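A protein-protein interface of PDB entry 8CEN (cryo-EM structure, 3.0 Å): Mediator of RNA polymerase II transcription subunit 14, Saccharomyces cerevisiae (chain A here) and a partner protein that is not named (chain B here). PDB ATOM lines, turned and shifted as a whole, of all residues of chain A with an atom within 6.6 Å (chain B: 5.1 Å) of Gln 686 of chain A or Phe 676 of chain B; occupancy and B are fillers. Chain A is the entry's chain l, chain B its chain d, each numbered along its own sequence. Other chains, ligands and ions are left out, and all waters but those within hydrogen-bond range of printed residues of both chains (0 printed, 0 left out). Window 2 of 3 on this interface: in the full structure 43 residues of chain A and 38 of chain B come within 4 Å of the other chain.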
ATOM      1  N   THR A 572      10.001  -4.899 -17.619  1.00  0.00           N
ATOM      2  CA  THR A 572       9.725  -3.656 -18.323  1.00  0.00           C
ATOM      3  C   THR A 572       9.826  -3.776 -19.840  1.00  0.00           C
ATOM      4  O   THR A 572       9.463  -2.826 -20.541  1.00  0.00           O
ATOM      5  CB  THR A 572      10.668  -2.557 -17.825  1.00  0.00           C
ATOM      6  OG1 THR A 572      12.022  -2.938 -18.085  1.00  0.00           O
ATOM      7  CG2 THR A 572      10.485  -2.335 -16.330  1.00  0.00           C
ATOM      8  N   THR A 684      18.175   1.123 -10.149  1.00  0.00           N
ATOM      9  CA  THR A 684      16.735   1.075  -9.929  1.00  0.00           C
ATOM     10  C   THR A 684      16.026   1.180 -11.273  1.00  0.00           C
ATOM     11  O   THR A 684      16.650   1.436 -12.305  1.00  0.00           O
ATOM     12  CB  THR A 684      16.274   2.188  -8.981  1.00  0.00           C
ATOM     13  OG1 THR A 684      14.847   2.158  -8.865  1.00  0.00           O
ATOM     14  CG2 THR A 684      16.710   3.547  -9.505  1.00  0.00           C
ATOM     15  N   TYR A 685      14.699   0.990 -11.241  1.00  0.00           N
ATOM     16  CA  TYR A 685      13.897   0.974 -12.465  1.00  0.00           C
ATOM     17  C   TYR A 685      13.921   2.309 -13.201  1.00  0.00           C
ATOM     18  O   TYR A 685      13.850   2.333 -14.437  1.00  0.00           O
ATOM     19  CB  TYR A 685      12.445   0.618 -12.154  1.00  0.00           C
ATOM     20  CG  TYR A 685      12.162  -0.801 -11.734  1.00  0.00           C
ATOM     21  CD1 TYR A 685      12.406  -1.862 -12.592  1.00  0.00           C
ATOM     22  CD2 TYR A 685      11.604  -1.074 -10.494  1.00  0.00           C
ATOM     23  CE1 TYR A 685      12.123  -3.158 -12.216  1.00  0.00           C
ATOM     24  CE2 TYR A 685      11.321  -2.367 -10.110  1.00  0.00           C
ATOM     25  CZ  TYR A 685      11.587  -3.406 -10.973  1.00  0.00           C
ATOM     26  OH  TYR A 685      11.307  -4.699 -10.594  1.00  0.00           O
ATOM     27  N   GLN A 686      13.975   3.423 -12.464  1.00  0.00           N
ATOM     28  CA  GLN A 686      14.042   4.734 -13.105  1.00  0.00           C
ATOM     29  C   GLN A 686      15.321   4.876 -13.919  1.00  0.00           C
ATOM     30  O   GLN A 686      15.301   5.393 -15.043  1.00  0.00           O
ATOM     31  CB  GLN A 686      13.952   5.840 -12.052  1.00  0.00           C
ATOM     32  CG  GLN A 686      13.146   5.478 -10.811  1.00  0.00           C
ATOM     33  CD  GLN A 686      11.650   5.443 -11.060  1.00  0.00           C
ATOM     34  OE1 GLN A 686      11.158   5.974 -12.057  1.00  0.00           O
ATOM     35  NE2 GLN A 686      10.915   4.830 -10.140  1.00  0.00           N
ATOM     36  N   LYS A 687      16.440   4.395 -13.373  1.00  0.00           N
ATOM     37  CA  LYS A 687      17.688   4.387 -14.124  1.00  0.00           C
ATOM     38  C   LYS A 687      17.615   3.434 -15.313  1.00  0.00           C
ATOM     39  O   LYS A 687      18.267   3.671 -16.330  1.00  0.00           O
ATOM     40  CB  LYS A 687      18.850   4.020 -13.200  1.00  0.00           C
ATOM     41  CG  LYS A 687      20.228   4.255 -13.800  1.00  0.00           C
ATOM     42  CD  LYS A 687      21.252   4.562 -12.719  1.00  0.00           C
ATOM     43  CE  LYS A 687      22.612   4.870 -13.321  1.00  0.00           C
ATOM     44  NZ  LYS A 687      22.545   6.001 -14.286  1.00  0.00           N
ATOM     45  N   ILE A 688      16.800   2.380 -15.223  1.00  0.00           N
ATOM     46  CA  ILE A 688      16.603   1.488 -16.365  1.00  0.00           C
ATOM     47  C   ILE A 688      15.815   2.192 -17.472  1.00  0.00           C
ATOM     48  O   ILE A 688      16.087   2.004 -18.665  1.00  0.00           O
ATOM     49  CB  ILE A 688      15.928   0.182 -15.903  1.00  0.00           C
ATOM     50  CG1 ILE A 688      16.784  -0.511 -14.843  1.00  0.00           C
ATOM     51  CG2 ILE A 688      15.744  -0.774 -17.051  1.00  0.00           C
ATOM     52  CD1 ILE A 688      18.161  -0.915 -15.331  1.00  0.00           C
ATOM     53  N   MET A 689      14.832   3.019 -17.101  1.00  0.00           N
ATOM     54  CA  MET A 689      14.111   3.793 -18.112  1.00  0.00           C
ATOM     55  C   MET A 689      15.003   4.858 -18.745  1.00  0.00           C
ATOM     56  O   MET A 689      14.920   5.109 -19.955  1.00  0.00           O
ATOM     57  CB  MET A 689      12.857   4.421 -17.509  1.00  0.00           C
ATOM     58  CG  MET A 689      11.780   3.409 -17.172  1.00  0.00           C
ATOM     59  SD  MET A 689      11.015   2.757 -18.671  1.00  0.00           S
ATOM     60  CE  MET A 689       9.318   2.559 -18.143  1.00  0.00           C
ATOM     61  N   ILE A 690      15.868   5.490 -17.945  1.00  0.00           N
ATOM     62  CA  ILE A 690      16.865   6.402 -18.509  1.00  0.00           C
ATOM     63  C   ILE A 690      17.835   5.640 -19.410  1.00  0.00           C
ATOM     64  O   ILE A 690      18.292   6.163 -20.435  1.00  0.00           O
ATOM     65  CB  ILE A 690      17.596   7.167 -17.384  1.00  0.00           C
ATOM     66  CG1 ILE A 690      16.592   7.922 -16.509  1.00  0.00           C
ATOM     67  CG2 ILE A 690      18.610   8.152 -17.946  1.00  0.00           C
ATOM     68  CD1 ILE A 690      15.696   8.871 -17.278  1.00  0.00           C
ATOM     69  N   LEU A 691      18.144   4.390 -19.056  1.00  0.00           N
ATOM     70  CA  LEU A 691      18.985   3.548 -19.901  1.00  0.00           C
ATOM     71  C   LEU A 691      18.324   3.273 -21.246  1.00  0.00           C
ATOM     72  O   LEU A 691      18.995   3.289 -22.281  1.00  0.00           O
ATOM     73  CB  LEU A 691      19.300   2.240 -19.176  1.00  0.00           C
ATOM     74  CG  LEU A 691      20.216   1.251 -19.895  1.00  0.00           C
ATOM     75  CD1 LEU A 691      21.589   1.864 -20.062  1.00  0.00           C
ATOM     76  CD2 LEU A 691      20.296  -0.062 -19.133  1.00  0.00           C
ATOM     77  N   ARG A 693      16.131   5.339 -22.631  1.00  0.00           N
ATOM     78  CA  ARG A 693      16.163   6.611 -23.346  1.00  0.00           C
ATOM     79  C   ARG A 693      17.567   7.009 -23.795  1.00  0.00           C
ATOM     80  O   ARG A 693      17.700   7.947 -24.590  1.00  0.00           O
ATOM     81  CB  ARG A 693      15.543   7.706 -22.479  1.00  0.00           C
ATOM     82  CG  ARG A 693      14.030   7.575 -22.357  1.00  0.00           C
ATOM     83  CD  ARG A 693      13.507   8.071 -21.022  1.00  0.00           C
ATOM     84  NE  ARG A 693      12.156   7.580 -20.770  1.00  0.00           N
ATOM     85  CZ  ARG A 693      11.480   7.784 -19.649  1.00  0.00           C
ATOM     86  NH1 ARG A 693      11.999   8.465 -18.642  1.00  0.00           N
ATOM     87  NH2 ARG A 693      10.250   7.290 -19.536  1.00  0.00           N
ATOM     88  N   ASP B 672       8.624  -2.862  -4.648  1.00  0.00           N
ATOM     89  CA  ASP B 672       9.206  -1.868  -5.542  1.00  0.00           C
ATOM     90  C   ASP B 672       8.605  -1.921  -6.942  1.00  0.00           C
ATOM     91  O   ASP B 672       8.591  -0.890  -7.624  1.00  0.00           O
ATOM     92  CB  ASP B 672      10.730  -2.019  -5.608  1.00  0.00           C
ATOM     93  CG  ASP B 672      11.170  -3.371  -6.121  1.00  0.00           C
ATOM     94  OD1 ASP B 672      10.978  -4.371  -5.413  1.00  0.00           O
ATOM     95  OD2 ASP B 672      11.743  -3.433  -7.224  1.00  0.00           O
ATOM     96  N   PHE B 673       8.069  -3.071  -7.377  1.00  0.00           N
ATOM     97  CA  PHE B 673       7.390  -3.090  -8.671  1.00  0.00           C
ATOM     98  C   PHE B 673       6.101  -2.273  -8.636  1.00  0.00           C
ATOM     99  O   PHE B 673       5.820  -1.509  -9.568  1.00  0.00           O
ATOM    100  CB  PHE B 673       7.102  -4.525  -9.106  1.00  0.00           C
ATOM    101  CG  PHE B 673       6.837  -4.664 -10.578  1.00  0.00           C
ATOM    102  CD1 PHE B 673       7.817  -4.345 -11.507  1.00  0.00           C
ATOM    103  CD2 PHE B 673       5.602  -5.096 -11.033  1.00  0.00           C
ATOM    104  CE1 PHE B 673       7.572  -4.469 -12.864  1.00  0.00           C
ATOM    105  CE2 PHE B 673       5.351  -5.222 -12.387  1.00  0.00           C
ATOM    106  CZ  PHE B 673       6.337  -4.908 -13.303  1.00  0.00           C
ATOM    107  N   LEU B 674       5.315  -2.409  -7.562  1.00  0.00           N
ATOM    108  CA  LEU B 674       4.119  -1.587  -7.404  1.00  0.00           C
ATOM    109  C   LEU B 674       4.480  -0.117  -7.248  1.00  0.00           C
ATOM    110  O   LEU B 674       3.764   0.761  -7.750  1.00  0.00           O
ATOM    111  CB  LEU B 674       3.309  -2.062  -6.198  1.00  0.00           C
ATOM    112  CG  LEU B 674       2.425  -3.295  -6.382  1.00  0.00           C
ATOM    113  CD1 LEU B 674       1.897  -3.774  -5.039  1.00  0.00           C
ATOM    114  CD2 LEU B 674       1.281  -2.990  -7.331  1.00  0.00           C
ATOM    115  N   HIS B 675       5.585   0.169  -6.550  1.00  0.00           N
ATOM    116  CA  HIS B 675       6.038   1.551  -6.409  1.00  0.00           C
ATOM    117  C   HIS B 675       6.395   2.162  -7.759  1.00  0.00           C
ATOM    118  O   HIS B 675       6.017   3.304  -8.049  1.00  0.00           O
ATOM    119  CB  HIS B 675       7.231   1.621  -5.458  1.00  0.00           C
ATOM    120  CG  HIS B 675       7.439   2.974  -4.856  1.00  0.00           C
ATOM    121  ND1 HIS B 675       8.540   3.287  -4.089  1.00  0.00           N
ATOM    122  CD2 HIS B 675       6.686   4.099  -4.909  1.00  0.00           C
ATOM    123  CE1 HIS B 675       8.456   4.545  -3.695  1.00  0.00           C
ATOM    124  NE2 HIS B 675       7.341   5.061  -4.180  1.00  0.00           N
ATOM    125  N   PHE B 676       7.107   1.413  -8.607  1.00  0.00           N
ATOM    126  CA  PHE B 676       7.419   1.917  -9.942  1.00  0.00           C
ATOM    127  C   PHE B 676       6.176   2.067 -10.808  1.00  0.00           C
ATOM    128  O   PHE B 676       6.081   3.016 -11.591  1.00  0.00           O
ATOM    129  CB  PHE B 676       8.447   1.032 -10.638  1.00  0.00           C
ATOM    130  CG  PHE B 676       8.818   1.524 -12.009  1.00  0.00           C
ATOM    131  CD1 PHE B 676       9.649   2.619 -12.168  1.00  0.00           C
ATOM    132  CD2 PHE B 676       8.350   0.872 -13.140  1.00  0.00           C
ATOM    133  CE1 PHE B 676       9.993   3.068 -13.429  1.00  0.00           C
ATOM    134  CE2 PHE B 676       8.691   1.314 -14.403  1.00  0.00           C
ATOM    135  CZ  PHE B 676       9.513   2.413 -14.547  1.00  0.00           C
ATOM    136  N   ILE B 677       5.223   1.137 -10.695  1.00  0.00           N
ATOM    137  CA  ILE B 677       3.996   1.237 -11.487  1.00  0.00           C
ATOM    138  C   ILE B 677       3.220   2.496 -11.111  1.00  0.00           C
ATOM    139  O   ILE B 677       2.826   3.290 -11.980  1.00  0.00           O
ATOM    140  CB  ILE B 677       3.143  -0.034 -11.317  1.00  0.00           C
ATOM    141  CG1 ILE B 677       3.756  -1.197 -12.102  1.00  0.00           C
ATOM    142  CG2 ILE B 677       1.706   0.211 -11.756  1.00  0.00           C
ATOM    143  CD1 ILE B 677       2.949  -2.480 -12.036  1.00  0.00           C
ATOM    144  N   VAL B 678       3.051   2.732  -9.806  1.00  0.00           N
ATOM    145  CA  VAL B 678       2.292   3.895  -9.354  1.00  0.00           C
ATOM    146  C   VAL B 678       3.076   5.196  -9.527  1.00  0.00           C
ATOM    147  O   VAL B 678       2.466   6.270  -9.599  1.00  0.00           O
ATOM    148  CB  VAL B 678       1.842   3.696  -7.892  1.00  0.00           C
ATOM    149  CG1 VAL B 678       2.997   3.899  -6.918  1.00  0.00           C
ATOM    150  CG2 VAL B 678       0.654   4.593  -7.547  1.00  0.00           C
ATOM    151  N   ALA B 679       4.405   5.137  -9.631  1.00  0.00           N
ATOM    152  CA  ALA B 679       5.185   6.348  -9.853  1.00  0.00           C
ATOM    153  C   ALA B 679       5.348   6.685 -11.327  1.00  0.00           C
ATOM    154  O   ALA B 679       5.568   7.854 -11.665  1.00  0.00           O
ATOM    155  CB  ALA B 679       6.565   6.214  -9.204  1.00  0.00           C
ATOM    156  N   GLU B 680       5.249   5.694 -12.212  1.00  0.00           N
ATOM    157  CA  GLU B 680       5.468   5.903 -13.637  1.00  0.00           C
ATOM    158  C   GLU B 680       4.179   6.088 -14.426  1.00  0.00           C
ATOM    159  O   GLU B 680       4.121   6.960 -15.298  1.00  0.00           O
ATOM    160  CB  GLU B 680       6.255   4.725 -14.222  1.00  0.00           C
ATOM    161  CG  GLU B 680       6.669   4.901 -15.675  1.00  0.00           C
ATOM    162  CD  GLU B 680       7.706   5.990 -15.859  1.00  0.00           C
ATOM    163  OE1 GLU B 680       8.637   6.072 -15.029  1.00  0.00           O
ATOM    164  OE2 GLU B 680       7.590   6.766 -16.830  1.00  0.00           O
ATOM    165  N   TYR B 681       3.138   5.302 -14.151  1.00  0.00           N
ATOM    166  CA  TYR B 681       1.952   5.328 -15.001  1.00  0.00           C
ATOM    167  C   TYR B 681       0.701   5.851 -14.317  1.00  0.00           C
ATOM    168  O   TYR B 681      -0.054   6.607 -14.934  1.00  0.00           O
ATOM    169  CB  TYR B 681       1.673   3.930 -15.564  1.00  0.00           C
ATOM    170  CG  TYR B 681       2.887   3.264 -16.170  1.00  0.00           C
ATOM    171  CD1 TYR B 681       3.277   3.550 -17.473  1.00  0.00           C
ATOM    172  CD2 TYR B 681       3.641   2.350 -15.446  1.00  0.00           C
ATOM    173  CE1 TYR B 681       4.386   2.946 -18.037  1.00  0.00           C
ATOM    174  CE2 TYR B 681       4.752   1.741 -16.000  1.00  0.00           C
ATOM    175  CZ  TYR B 681       5.118   2.042 -17.296  1.00  0.00           C
ATOM    176  OH  TYR B 681       6.220   1.438 -17.851  1.00  0.00           O
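Gln 686 of chain A touches two residues of chain B. Phe 676 of chain B touches just these residues of chain A: Tyr 685, Gln 686 and Met 689. Of the printed residues of chain B, Tyr 685 of chain A touches Asp 672 (3.1 Å), Phe 673 (3.6 Å) and Phe 676 (3.4 Å). Of the printed residues of chain A, Phe 673 of chain B touches Tyr 685. Of the printed residues of chain A, Tyr 681 of chain B touches Met 689. Of the printed residues of chain B, Met 689 of chain A touches Phe 676 and Tyr 681. Of the printed residues of chain B, Arg 693 of chain A touches Glu 680 (3.8 Å). The nearest residue of chain B that does not touch Gln 686 of chain A is Ala 679 of chain B (4.7 Å). The nearest printed residue of chain B that does not touch Tyr 685 of chain A is Glu 680 of chain B (6.4 Å).
Hydrophobic or aromatic side chains of chain B within 4 Å of the printed part of chain A: Phe 673, Phe 676 and Tyr 681. Of the 10 printed residues of chain A, 4 touch a printed residue of chain B. Hydrophobic or aromatic side chains of chain A that line the printed part of chain B: Tyr 685 and Met 689. Among the printed residues, 8 pairs touch across the chains.
CE2 of Tyr 685 of chain A touches OD2 of Asp 672 of chain B (3.1 Å). OH of Tyr 685 of chain A touches CD1 of Phe 673 of chain B, at 3.6 Å. Phe 676 of chain B touches Tyr 685 of chain A (CD1 to CB, 3.4 Å). Phe 676 of chain B touches Gln 686 of chain A (CD1 to NE2, 3.3 Å). Glu 680 of chain B touches Gln 686 of chain A. Phe 676 of chain B touches Met 689 of chain A (CZ to CE, 3.6 Å). Met 689 of chain A touches Tyr 681 of chain B.
OE2 of Glu 680 of chain B is in salt-bridge range of NH2 of Arg 693 of chain A, 3.8 Å away.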
